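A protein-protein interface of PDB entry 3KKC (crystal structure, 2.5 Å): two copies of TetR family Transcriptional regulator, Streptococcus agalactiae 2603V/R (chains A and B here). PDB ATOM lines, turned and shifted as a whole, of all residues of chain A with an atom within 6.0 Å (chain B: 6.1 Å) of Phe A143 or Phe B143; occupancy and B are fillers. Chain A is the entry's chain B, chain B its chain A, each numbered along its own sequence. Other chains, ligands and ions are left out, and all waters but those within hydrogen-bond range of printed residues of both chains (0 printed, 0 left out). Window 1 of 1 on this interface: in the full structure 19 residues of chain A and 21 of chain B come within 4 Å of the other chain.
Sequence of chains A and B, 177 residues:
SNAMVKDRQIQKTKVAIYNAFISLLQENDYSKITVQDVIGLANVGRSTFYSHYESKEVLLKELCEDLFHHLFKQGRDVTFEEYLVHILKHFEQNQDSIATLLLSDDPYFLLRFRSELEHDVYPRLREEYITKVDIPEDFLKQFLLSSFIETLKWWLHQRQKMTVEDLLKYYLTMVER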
ATOM      1  N   ASP A 138      20.514  23.796 -17.300  1.00  0.00           N
ATOM      2  CA  ASP A 138      21.231  23.782 -16.021  1.00  0.00           C
ATOM      3  C   ASP A 138      20.475  24.537 -14.927  1.00  0.00           C
ATOM      4  O   ASP A 138      20.345  24.043 -13.811  1.00  0.00           O
ATOM      5  CB  ASP A 138      22.654  24.327 -16.174  1.00  0.00           C
ATOM      6  CG  ASP A 138      22.687  25.789 -16.618  1.00  0.00           C
ATOM      7  OD1 ASP A 138      21.696  26.277 -17.217  1.00  0.00           O
ATOM      8  OD2 ASP A 138      23.716  26.454 -16.362  1.00  0.00           O
ATOM      9  N   PHE A 139      19.955  25.719 -15.240  1.00  0.00           N
ATOM     10  CA  PHE A 139      19.158  26.433 -14.257  1.00  0.00           C
ATOM     11  C   PHE A 139      17.944  25.591 -13.886  1.00  0.00           C
ATOM     12  O   PHE A 139      17.639  25.406 -12.708  1.00  0.00           O
ATOM     13  CB  PHE A 139      18.704  27.782 -14.780  1.00  0.00           C
ATOM     14  CG  PHE A 139      18.017  28.610 -13.752  1.00  0.00           C
ATOM     15  CD1 PHE A 139      18.742  29.387 -12.877  1.00  0.00           C
ATOM     16  CD2 PHE A 139      16.655  28.592 -13.635  1.00  0.00           C
ATOM     17  CE1 PHE A 139      18.104  30.137 -11.912  1.00  0.00           C
ATOM     18  CE2 PHE A 139      16.017  29.345 -12.677  1.00  0.00           C
ATOM     19  CZ  PHE A 139      16.736  30.110 -11.817  1.00  0.00           C
ATOM     20  N   LEU A 140      17.267  25.066 -14.908  1.00  0.00           N
ATOM     21  CA  LEU A 140      16.104  24.202 -14.724  1.00  0.00           C
ATOM     22  C   LEU A 140      16.404  23.057 -13.759  1.00  0.00           C
ATOM     23  O   LEU A 140      15.623  22.793 -12.856  1.00  0.00           O
ATOM     24  CB  LEU A 140      15.645  23.640 -16.069  1.00  0.00           C
ATOM     25  CG  LEU A 140      14.146  23.549 -16.359  1.00  0.00           C
ATOM     26  CD1 LEU A 140      13.318  23.935 -15.142  1.00  0.00           C
ATOM     27  CD2 LEU A 140      13.790  24.431 -17.529  1.00  0.00           C
ATOM     28  N   LYS A 141      17.541  22.396 -13.966  1.00  0.00           N
ATOM     29  CA  LYS A 141      17.961  21.205 -13.209  1.00  0.00           C
ATOM     30  C   LYS A 141      18.307  21.513 -11.761  1.00  0.00           C
ATOM     31  O   LYS A 141      17.875  20.818 -10.838  1.00  0.00           O
ATOM     32  CB  LYS A 141      19.185  20.573 -13.878  1.00  0.00           C
ATOM     33  CG  LYS A 141      19.622  19.237 -13.306  1.00  0.00           C
ATOM     34  CD  LYS A 141      20.692  18.577 -14.181  1.00  0.00           C
ATOM     35  CE  LYS A 141      21.464  17.507 -13.415  1.00  0.00           C
ATOM     36  NZ  LYS A 141      22.725  17.122 -14.114  1.00  0.00           N
ATOM     37  N   GLN A 142      19.111  22.549 -11.567  1.00  0.00           N
ATOM     38  CA  GLN A 142      19.435  23.003 -10.226  1.00  0.00           C
ATOM     39  C   GLN A 142      18.174  23.340  -9.414  1.00  0.00           C
ATOM     40  O   GLN A 142      18.084  23.050  -8.224  1.00  0.00           O
ATOM     41  CB  GLN A 142      20.361  24.215 -10.301  1.00  0.00           C
ATOM     42  CG  GLN A 142      20.433  25.002  -9.018  1.00  0.00           C
ATOM     43  CD  GLN A 142      19.351  26.030  -8.956  1.00  0.00           C
ATOM     44  OE1 GLN A 142      19.061  26.689  -9.956  1.00  0.00           O
ATOM     45  NE2 GLN A 142      18.727  26.176  -7.781  1.00  0.00           N
ATOM     46  N   PHE A 143      17.201  23.953 -10.068  1.00  0.00           N
ATOM     47  CA  PHE A 143      16.029  24.471  -9.377  1.00  0.00           C
ATOM     48  C   PHE A 143      15.045  23.389  -8.931  1.00  0.00           C
ATOM     49  O   PHE A 143      14.491  23.461  -7.835  1.00  0.00           O
ATOM     50  CB  PHE A 143      15.310  25.447 -10.298  1.00  0.00           C
ATOM     51  CG  PHE A 143      14.126  26.098  -9.677  1.00  0.00           C
ATOM     52  CD1 PHE A 143      14.261  27.291  -8.994  1.00  0.00           C
ATOM     53  CD2 PHE A 143      12.870  25.524  -9.786  1.00  0.00           C
ATOM     54  CE1 PHE A 143      13.161  27.905  -8.430  1.00  0.00           C
ATOM     55  CE2 PHE A 143      11.763  26.132  -9.221  1.00  0.00           C
ATOM     56  CZ  PHE A 143      11.903  27.334  -8.553  1.00  0.00           C
ATOM     57  N   LEU A 144      14.820  22.410  -9.806  1.00  0.00           N
ATOM     58  CA  LEU A 144      13.916  21.296  -9.551  1.00  0.00           C
ATOM     59  C   LEU A 144      14.439  20.428  -8.406  1.00  0.00           C
ATOM     60  O   LEU A 144      13.744  20.214  -7.416  1.00  0.00           O
ATOM     61  CB  LEU A 144      13.765  20.450 -10.821  1.00  0.00           C
ATOM     62  CG  LEU A 144      12.493  20.592 -11.680  1.00  0.00           C
ATOM     63  CD1 LEU A 144      11.595  21.699 -11.197  1.00  0.00           C
ATOM     64  CD2 LEU A 144      12.793  20.754 -13.174  1.00  0.00           C
ATOM     65  N   LEU A 145      15.672  19.941  -8.563  1.00  0.00           N
ATOM     66  CA  LEU A 145      16.383  19.149  -7.547  1.00  0.00           C
ATOM     67  C   LEU A 145      16.440  19.796  -6.149  1.00  0.00           C
ATOM     68  O   LEU A 145      16.123  19.144  -5.160  1.00  0.00           O
ATOM     69  CB  LEU A 145      17.800  18.810  -8.032  1.00  0.00           C
ATOM     70  CG  LEU A 145      18.080  17.403  -8.584  1.00  0.00           C
ATOM     71  CD1 LEU A 145      16.805  16.616  -8.893  1.00  0.00           C
ATOM     72  CD2 LEU A 145      19.024  17.464  -9.789  1.00  0.00           C
ATOM     73  N   SER A 146      16.842  21.062  -6.066  1.00  0.00           N
ATOM     74  CA  SER A 146      16.845  21.750  -4.789  1.00  0.00           C
ATOM     75  C   SER A 146      15.433  21.899  -4.247  1.00  0.00           C
ATOM     76  O   SER A 146      15.191  21.697  -3.054  1.00  0.00           O
ATOM     77  CB  SER A 146      17.507  23.133  -4.883  1.00  0.00           C
ATOM     78  OG  SER A 146      18.890  23.019  -5.168  1.00  0.00           O
ATOM     79  N   SER A 147      14.492  22.289  -5.096  1.00  0.00           N
ATOM     80  CA  SER A 147      13.126  22.459  -4.594  1.00  0.00           C
ATOM     81  C   SER A 147      12.610  21.128  -4.014  1.00  0.00           C
ATOM     82  O   SER A 147      11.961  21.100  -2.962  1.00  0.00           O
ATOM     83  CB  SER A 147      12.181  23.034  -5.654  1.00  0.00           C
ATOM     84  OG  SER A 147      12.119  22.203  -6.800  1.00  0.00           O
ATOM     85  N   PHE A 148      12.945  20.026  -4.674  1.00  0.00           N
ATOM     86  CA  PHE A 148      12.467  18.740  -4.213  1.00  0.00           C
ATOM     87  C   PHE A 148      13.049  18.422  -2.848  1.00  0.00           C
ATOM     88  O   PHE A 148      12.313  18.225  -1.882  1.00  0.00           O
ATOM     89  CB  PHE A 148      12.810  17.630  -5.208  1.00  0.00           C
ATOM     90  CG  PHE A 148      12.162  16.312  -4.883  1.00  0.00           C
ATOM     91  CD1 PHE A 148      10.798  16.133  -5.085  1.00  0.00           C
ATOM     92  CD2 PHE A 148      12.914  15.264  -4.371  1.00  0.00           C
ATOM     93  CE1 PHE A 148      10.195  14.939  -4.804  1.00  0.00           C
ATOM     94  CE2 PHE A 148      12.327  14.051  -4.079  1.00  0.00           C
ATOM     95  CZ  PHE A 148      10.956  13.886  -4.294  1.00  0.00           C
ATOM     96  N   THR A 151      11.870  20.801  -0.141  1.00  0.00           N
ATOM     97  CA  THR A 151      10.460  20.602   0.177  1.00  0.00           C
ATOM     98  C   THR A 151      10.391  19.311   1.000  1.00  0.00           C
ATOM     99  O   THR A 151       9.746  19.252   2.054  1.00  0.00           O
ATOM    100  CB  THR A 151       9.558  20.589  -1.099  1.00  0.00           C
ATOM    101  OG1 THR A 151       9.468  21.929  -1.616  1.00  0.00           O
ATOM    102  CG2 THR A 151       8.137  20.071  -0.801  1.00  0.00           C
ATOM    103  N   TYR A 171       3.799  20.284  -4.495  1.00  0.00           N
ATOM    104  CA  TYR A 171       5.113  20.384  -5.104  1.00  0.00           C
ATOM    105  C   TYR A 171       4.961  20.478  -6.606  1.00  0.00           C
ATOM    106  O   TYR A 171       5.507  21.377  -7.226  1.00  0.00           O
ATOM    107  CB  TYR A 171       5.988  19.183  -4.807  1.00  0.00           C
ATOM    108  CG  TYR A 171       7.285  19.281  -5.574  1.00  0.00           C
ATOM    109  CD1 TYR A 171       8.222  20.282  -5.283  1.00  0.00           C
ATOM    110  CD2 TYR A 171       7.583  18.388  -6.587  1.00  0.00           C
ATOM    111  CE1 TYR A 171       9.420  20.377  -5.988  1.00  0.00           C
ATOM    112  CE2 TYR A 171       8.769  18.467  -7.296  1.00  0.00           C
ATOM    113  CZ  TYR A 171       9.678  19.465  -6.995  1.00  0.00           C
ATOM    114  OH  TYR A 171      10.839  19.529  -7.715  1.00  0.00           O
ATOM    115  N   MET A 174       3.475  23.333  -8.362  1.00  0.00           N
ATOM    116  CA  MET A 174       4.356  24.486  -8.112  1.00  0.00           C
ATOM    117  C   MET A 174       5.468  24.629  -9.144  1.00  0.00           C
ATOM    118  O   MET A 174       5.895  25.750  -9.433  1.00  0.00           O
ATOM    119  CB  MET A 174       5.027  24.412  -6.730  1.00  0.00           C
ATOM    120  CG  MET A 174       4.572  25.416  -5.652  1.00  0.00           C
ATOM    121  SD  MET A 174       4.293  27.319  -6.083  1.00  0.00           S
ATOM    122  CE  MET A 174       6.056  28.027  -5.710  1.00  0.00           C
ATOM    123  N   VAL A 175       5.987  23.515  -9.652  1.00  0.00           N
ATOM    124  CA  VAL A 175       7.043  23.579 -10.656  1.00  0.00           C
ATOM    125  C   VAL A 175       6.503  23.465 -12.070  1.00  0.00           C
ATOM    126  O   VAL A 175       7.160  23.918 -13.013  1.00  0.00           O
ATOM    127  CB  VAL A 175       8.172  22.532 -10.445  1.00  0.00           C
ATOM    128  CG1 VAL A 175       8.756  22.650  -9.042  1.00  0.00           C
ATOM    129  CG2 VAL A 175       7.691  21.115 -10.718  1.00  0.00           C
ATOM    130  N   ASP B 138       1.842  28.464   3.872  1.00  0.00           N
ATOM    131  CA  ASP B 138       3.108  28.039   4.464  1.00  0.00           C
ATOM    132  C   ASP B 138       4.000  27.290   3.467  1.00  0.00           C
ATOM    133  O   ASP B 138       5.225  27.364   3.537  1.00  0.00           O
ATOM    134  CB  ASP B 138       2.885  27.249   5.762  1.00  0.00           C
ATOM    135  CG  ASP B 138       2.132  25.956   5.544  1.00  0.00           C
ATOM    136  OD1 ASP B 138       1.270  25.897   4.640  1.00  0.00           O
ATOM    137  OD2 ASP B 138       2.409  24.992   6.285  1.00  0.00           O
ATOM    138  N   PHE B 139       3.381  26.593   2.524  1.00  0.00           N
ATOM    139  CA  PHE B 139       4.139  25.854   1.540  1.00  0.00           C
ATOM    140  C   PHE B 139       4.701  26.859   0.576  1.00  0.00           C
ATOM    141  O   PHE B 139       5.820  26.724   0.081  1.00  0.00           O
ATOM    142  CB  PHE B 139       3.228  24.900   0.780  1.00  0.00           C
ATOM    143  CG  PHE B 139       3.958  24.003  -0.178  1.00  0.00           C
ATOM    144  CD1 PHE B 139       4.344  22.736   0.205  1.00  0.00           C
ATOM    145  CD2 PHE B 139       4.261  24.433  -1.448  1.00  0.00           C
ATOM    146  CE1 PHE B 139       5.008  21.922  -0.667  1.00  0.00           C
ATOM    147  CE2 PHE B 139       4.923  23.618  -2.324  1.00  0.00           C
ATOM    148  CZ  PHE B 139       5.298  22.366  -1.936  1.00  0.00           C
ATOM    149  N   LEU B 140       3.896  27.875   0.301  1.00  0.00           N
ATOM    150  CA  LEU B 140       4.332  28.986  -0.514  1.00  0.00           C
ATOM    151  C   LEU B 140       5.556  29.644   0.146  1.00  0.00           C
ATOM    152  O   LEU B 140       6.621  29.773  -0.473  1.00  0.00           O
ATOM    153  CB  LEU B 140       3.190  29.985  -0.698  1.00  0.00           C
ATOM    154  CG  LEU B 140       2.789  30.300  -2.141  1.00  0.00           C
ATOM    155  CD1 LEU B 140       3.073  29.130  -3.080  1.00  0.00           C
ATOM    156  CD2 LEU B 140       1.318  30.670  -2.186  1.00  0.00           C
ATOM    157  N   LYS B 141       5.420  30.039   1.407  1.00  0.00           N
ATOM    158  CA  LYS B 141       6.498  30.762   2.036  1.00  0.00           C
ATOM    159  C   LYS B 141       7.772  29.954   1.875  1.00  0.00           C
ATOM    160  O   LYS B 141       8.765  30.474   1.348  1.00  0.00           O
ATOM    161  CB  LYS B 141       6.209  31.047   3.502  1.00  0.00           C
ATOM    162  CG  LYS B 141       7.175  32.067   4.072  1.00  0.00           C
ATOM    163  CD  LYS B 141       6.937  32.296   5.549  1.00  0.00           C
ATOM    164  CE  LYS B 141       7.575  33.593   5.986  1.00  0.00           C
ATOM    165  NZ  LYS B 141       7.230  33.885   7.404  1.00  0.00           N
ATOM    166  N   GLN B 142       7.713  28.677   2.281  1.00  0.00           N
ATOM    167  CA  GLN B 142       8.883  27.791   2.302  1.00  0.00           C
ATOM    168  C   GLN B 142       9.487  27.492   0.916  1.00  0.00           C
ATOM    169  O   GLN B 142      10.701  27.486   0.733  1.00  0.00           O
ATOM    170  CB  GLN B 142       8.536  26.484   3.022  1.00  0.00           C
ATOM    171  CG  GLN B 142       9.482  25.312   2.725  1.00  0.00           C
ATOM    172  CD  GLN B 142       9.137  24.563   1.451  1.00  0.00           C
ATOM    173  OE1 GLN B 142       7.967  24.379   1.135  1.00  0.00           O
ATOM    174  NE2 GLN B 142      10.159  24.131   0.711  1.00  0.00           N
ATOM    175  N   PHE B 143       8.653  27.242  -0.076  1.00  0.00           N
ATOM    176  CA  PHE B 143       9.189  26.964  -1.404  1.00  0.00           C
ATOM    177  C   PHE B 143       9.899  28.183  -2.006  1.00  0.00           C
ATOM    178  O   PHE B 143      10.880  28.061  -2.740  1.00  0.00           O
ATOM    179  CB  PHE B 143       8.056  26.515  -2.312  1.00  0.00           C
ATOM    180  CG  PHE B 143       8.503  26.011  -3.665  1.00  0.00           C
ATOM    181  CD1 PHE B 143       8.583  24.645  -3.922  1.00  0.00           C
ATOM    182  CD2 PHE B 143       8.781  26.901  -4.700  1.00  0.00           C
ATOM    183  CE1 PHE B 143       8.966  24.172  -5.184  1.00  0.00           C
ATOM    184  CE2 PHE B 143       9.158  26.447  -5.964  1.00  0.00           C
ATOM    185  CZ  PHE B 143       9.253  25.088  -6.209  1.00  0.00           C
ATOM    186  N   LEU B 144       9.388  29.365  -1.690  1.00  0.00           N
ATOM    187  CA  LEU B 144       9.815  30.588  -2.354  1.00  0.00           C
ATOM    188  C   LEU B 144      11.154  31.068  -1.773  1.00  0.00           C
ATOM    189  O   LEU B 144      12.118  31.316  -2.510  1.00  0.00           O
ATOM    190  CB  LEU B 144       8.743  31.665  -2.175  1.00  0.00           C
ATOM    191  CG  LEU B 144       7.869  32.167  -3.321  1.00  0.00           C
ATOM    192  CD1 LEU B 144       8.076  31.378  -4.580  1.00  0.00           C
ATOM    193  CD2 LEU B 144       6.430  32.147  -2.889  1.00  0.00           C
ATOM    194  N   LEU B 145      11.193  31.196  -0.446  1.00  0.00           N
ATOM    195  CA  LEU B 145      12.374  31.656   0.263  1.00  0.00           C
ATOM    196  C   LEU B 145      13.521  30.707   0.029  1.00  0.00           C
ATOM    197  O   LEU B 145      14.625  31.127  -0.290  1.00  0.00           O
ATOM    198  CB  LEU B 145      12.095  31.762   1.759  1.00  0.00           C
ATOM    199  CG  LEU B 145      12.082  33.187   2.303  1.00  0.00           C
ATOM    200  CD1 LEU B 145      11.860  34.171   1.199  1.00  0.00           C
ATOM    201  CD2 LEU B 145      11.009  33.341   3.366  1.00  0.00           C
ATOM    202  N   SER B 146      13.252  29.416   0.170  1.00  0.00           N
ATOM    203  CA  SER B 146      14.306  28.431   0.035  1.00  0.00           C
ATOM    204  C   SER B 146      14.812  28.303  -1.402  1.00  0.00           C
ATOM    205  O   SER B 146      16.003  28.062  -1.626  1.00  0.00           O
ATOM    206  CB  SER B 146      13.852  27.071   0.563  1.00  0.00           C
ATOM    207  OG  SER B 146      14.331  26.053  -0.295  1.00  0.00           O
ATOM    208  N   SER B 147      13.925  28.448  -2.381  1.00  0.00           N
ATOM    209  CA  SER B 147      14.379  28.361  -3.765  1.00  0.00           C
ATOM    210  C   SER B 147      15.123  29.652  -4.177  1.00  0.00           C
ATOM    211  O   SER B 147      15.963  29.655  -5.084  1.00  0.00           O
ATOM    212  CB  SER B 147      13.205  28.112  -4.699  1.00  0.00           C
ATOM    213  OG  SER B 147      12.536  29.336  -4.950  1.00  0.00           O
ATOM    214  N   PHE B 148      14.813  30.759  -3.514  1.00  0.00           N
ATOM    215  CA  PHE B 148      15.588  31.960  -3.761  1.00  0.00           C
ATOM    216  C   PHE B 148      17.020  31.757  -3.253  1.00  0.00           C
ATOM    217  O   PHE B 148      17.974  31.897  -4.031  1.00  0.00           O
ATOM    218  CB  PHE B 148      14.934  33.200  -3.150  1.00  0.00           C
ATOM    219  CG  PHE B 148      15.739  34.455  -3.333  1.00  0.00           C
ATOM    220  CD1 PHE B 148      15.638  35.189  -4.495  1.00  0.00           C
ATOM    221  CD2 PHE B 148      16.602  34.894  -2.338  1.00  0.00           C
ATOM    222  CE1 PHE B 148      16.367  36.334  -4.658  1.00  0.00           C
ATOM    223  CE2 PHE B 148      17.328  36.036  -2.496  1.00  0.00           C
ATOM    224  CZ  PHE B 148      17.215  36.754  -3.652  1.00  0.00           C
ATOM    225  N   THR B 151      18.770  29.103  -5.478  1.00  0.00           N
ATOM    226  CA  THR B 151      19.160  29.591  -6.797  1.00  0.00           C
ATOM    227  C   THR B 151      20.463  30.369  -6.635  1.00  0.00           C
ATOM    228  O   THR B 151      21.452  30.099  -7.326  1.00  0.00           O
ATOM    229  CB  THR B 151      18.083  30.480  -7.451  1.00  0.00           C
ATOM    230  OG1 THR B 151      16.987  29.665  -7.864  1.00  0.00           O
ATOM    231  CG2 THR B 151      18.643  31.225  -8.684  1.00  0.00           C
ATOM    232  N   TYR B 171      14.598  33.171 -12.436  1.00  0.00           N
ATOM    233  CA  TYR B 171      14.031  32.779 -11.170  1.00  0.00           C
ATOM    234  C   TYR B 171      12.564  33.194 -11.066  1.00  0.00           C
ATOM    235  O   TYR B 171      11.704  32.404 -10.658  1.00  0.00           O
ATOM    236  CB  TYR B 171      14.845  33.348 -10.005  1.00  0.00           C
ATOM    237  CG  TYR B 171      14.126  33.188  -8.688  1.00  0.00           C
ATOM    238  CD1 TYR B 171      14.154  31.989  -7.997  1.00  0.00           C
ATOM    239  CD2 TYR B 171      13.372  34.227  -8.165  1.00  0.00           C
ATOM    240  CE1 TYR B 171      13.464  31.837  -6.799  1.00  0.00           C
ATOM    241  CE2 TYR B 171      12.691  34.084  -6.978  1.00  0.00           C
ATOM    242  CZ  TYR B 171      12.739  32.894  -6.296  1.00  0.00           C
ATOM    243  OH  TYR B 171      12.047  32.790  -5.109  1.00  0.00           O
ATOM    244  N   MET B 174      10.364  31.114 -13.144  1.00  0.00           N
ATOM    245  CA  MET B 174      10.257  29.782 -12.547  1.00  0.00           C
ATOM    246  C   MET B 174       9.236  29.707 -11.428  1.00  0.00           C
ATOM    247  O   MET B 174       8.599  28.675 -11.246  1.00  0.00           O
ATOM    248  CB  MET B 174      11.601  29.281 -12.043  1.00  0.00           C
ATOM    249  CG  MET B 174      12.399  28.537 -13.084  1.00  0.00           C
ATOM    250  SD  MET B 174      11.282  27.251 -14.014  1.00  0.00           S
ATOM    251  CE  MET B 174      10.934  26.011 -12.533  1.00  0.00           C
ATOM    252  N   VAL B 175       9.073  30.803 -10.693  1.00  0.00           N
ATOM    253  CA  VAL B 175       8.201  30.799  -9.521  1.00  0.00           C
ATOM    254  C   VAL B 175       6.833  31.437  -9.728  1.00  0.00           C
ATOM    255  O   VAL B 175       5.884  31.091  -9.037  1.00  0.00           O
ATOM    256  CB  VAL B 175       8.871  31.495  -8.338  1.00  0.00           C
ATOM    257  CG1 VAL B 175      10.145  30.763  -7.968  1.00  0.00           C
ATOM    258  CG2 VAL B 175       9.167  32.936  -8.677  1.00  0.00           C
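Phe B143 touches its own counterpart, Phe A143.
Phe A143 touches Ser B147, and with the chains exchanged Ser A147 touches Phe B143.
Phe A143 touches Met B174, and with the chains exchanged Met A174 touches Phe B143.
Phe A143 touches Val B175, and with the chains exchanged Val A175 touches Phe B143.
Positions printed for both chains: 138, 139, 140, 141, 142, 143, 144, 145, 146, 147, 148, 151, 171, 174 and 175.
Of the 19 pairs that touch across the chains among the printed residues, 17 have their exchanged pair printed and touching as well.
The side-chain amide nitrogen of Gln B142 lies within hydrogen-bond range of the side-chain hydroxyl of Thr A151 (3.3 Å).
CG2 of Thr B151 touches CE1 of Phe A139 (3.4 Å).
Thr B151 touches Gln A142.
CB of Ser B147 touches CE1 of Phe A143, at 3.7 Å.
OG1 of Thr B151 touches CD1 of Phe A143, 3.8 Å away.
Met B174 touches Phe A143.
Phe B139 touches Thr A151 (CE1 to CG2, 3.6 Å).
CD1 of Phe B143 touches OG1 of Thr A151, 3.7 Å away.
Tyr A171 touches Phe B139 (N to CZ, 3.6 Å).
CG of Met A174 touches CE2 of Phe B139 (3.8 Å).
Leu B140 touches Met A174 (CD1 to SD, 3.7 Å).
Of the 15 printed residues of chain A, 8 touch a printed residue of chain B.
Along chain A the printed residues that touch a printed residue of chain B span positions 139 to 175.
Of the 15 printed residues of chain B, 9 touch a printed residue of chain A.
Phe A143 touches five residues of chain B.
Phe B143 touches just these residues of chain A: Phe A143, Ser A147, Thr A151, Tyr A171, Met A174 and Val A175.
Of the printed residues of chain A, Leu B140 touches Met A174.
Printed residues of chain A within 4 Å of Tyr B171: Phe A139.
The nearest residue of chain B that does not touch Phe A143 is Tyr B171 (4.2 Å).
The nearest residue of chain A that does not touch Phe B143 is Phe A148 (5.8 Å).
The backbone carbonyl oxygen (O) of Phe B139 sits close to the side-chain amide oxygen (OE1) of Gln B142.
The side-chain hydroxyl of Ser B147 is in hydrogen-bond range of the backbone carbonyl oxygen of Leu B144 (3.2 Å).
The backbone carbonyl oxygen (O) of Ser B147 is in hydrogen-bond range of the side-chain hydroxyl (OG1) of Thr B151.
The backbone carbonyl oxygen of Phe A139 sits close to the side-chain amide oxygen of Gln A142 (3.4 Å).
The backbone carbonyl oxygen (O) of Leu A144 is in hydrogen-bond range of the side-chain hydroxyl (OG) of Ser A147, 2.6 Å away.
OG of Ser A147 lies within hydrogen-bond range of OH of Tyr A171, 3.1 Å away.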
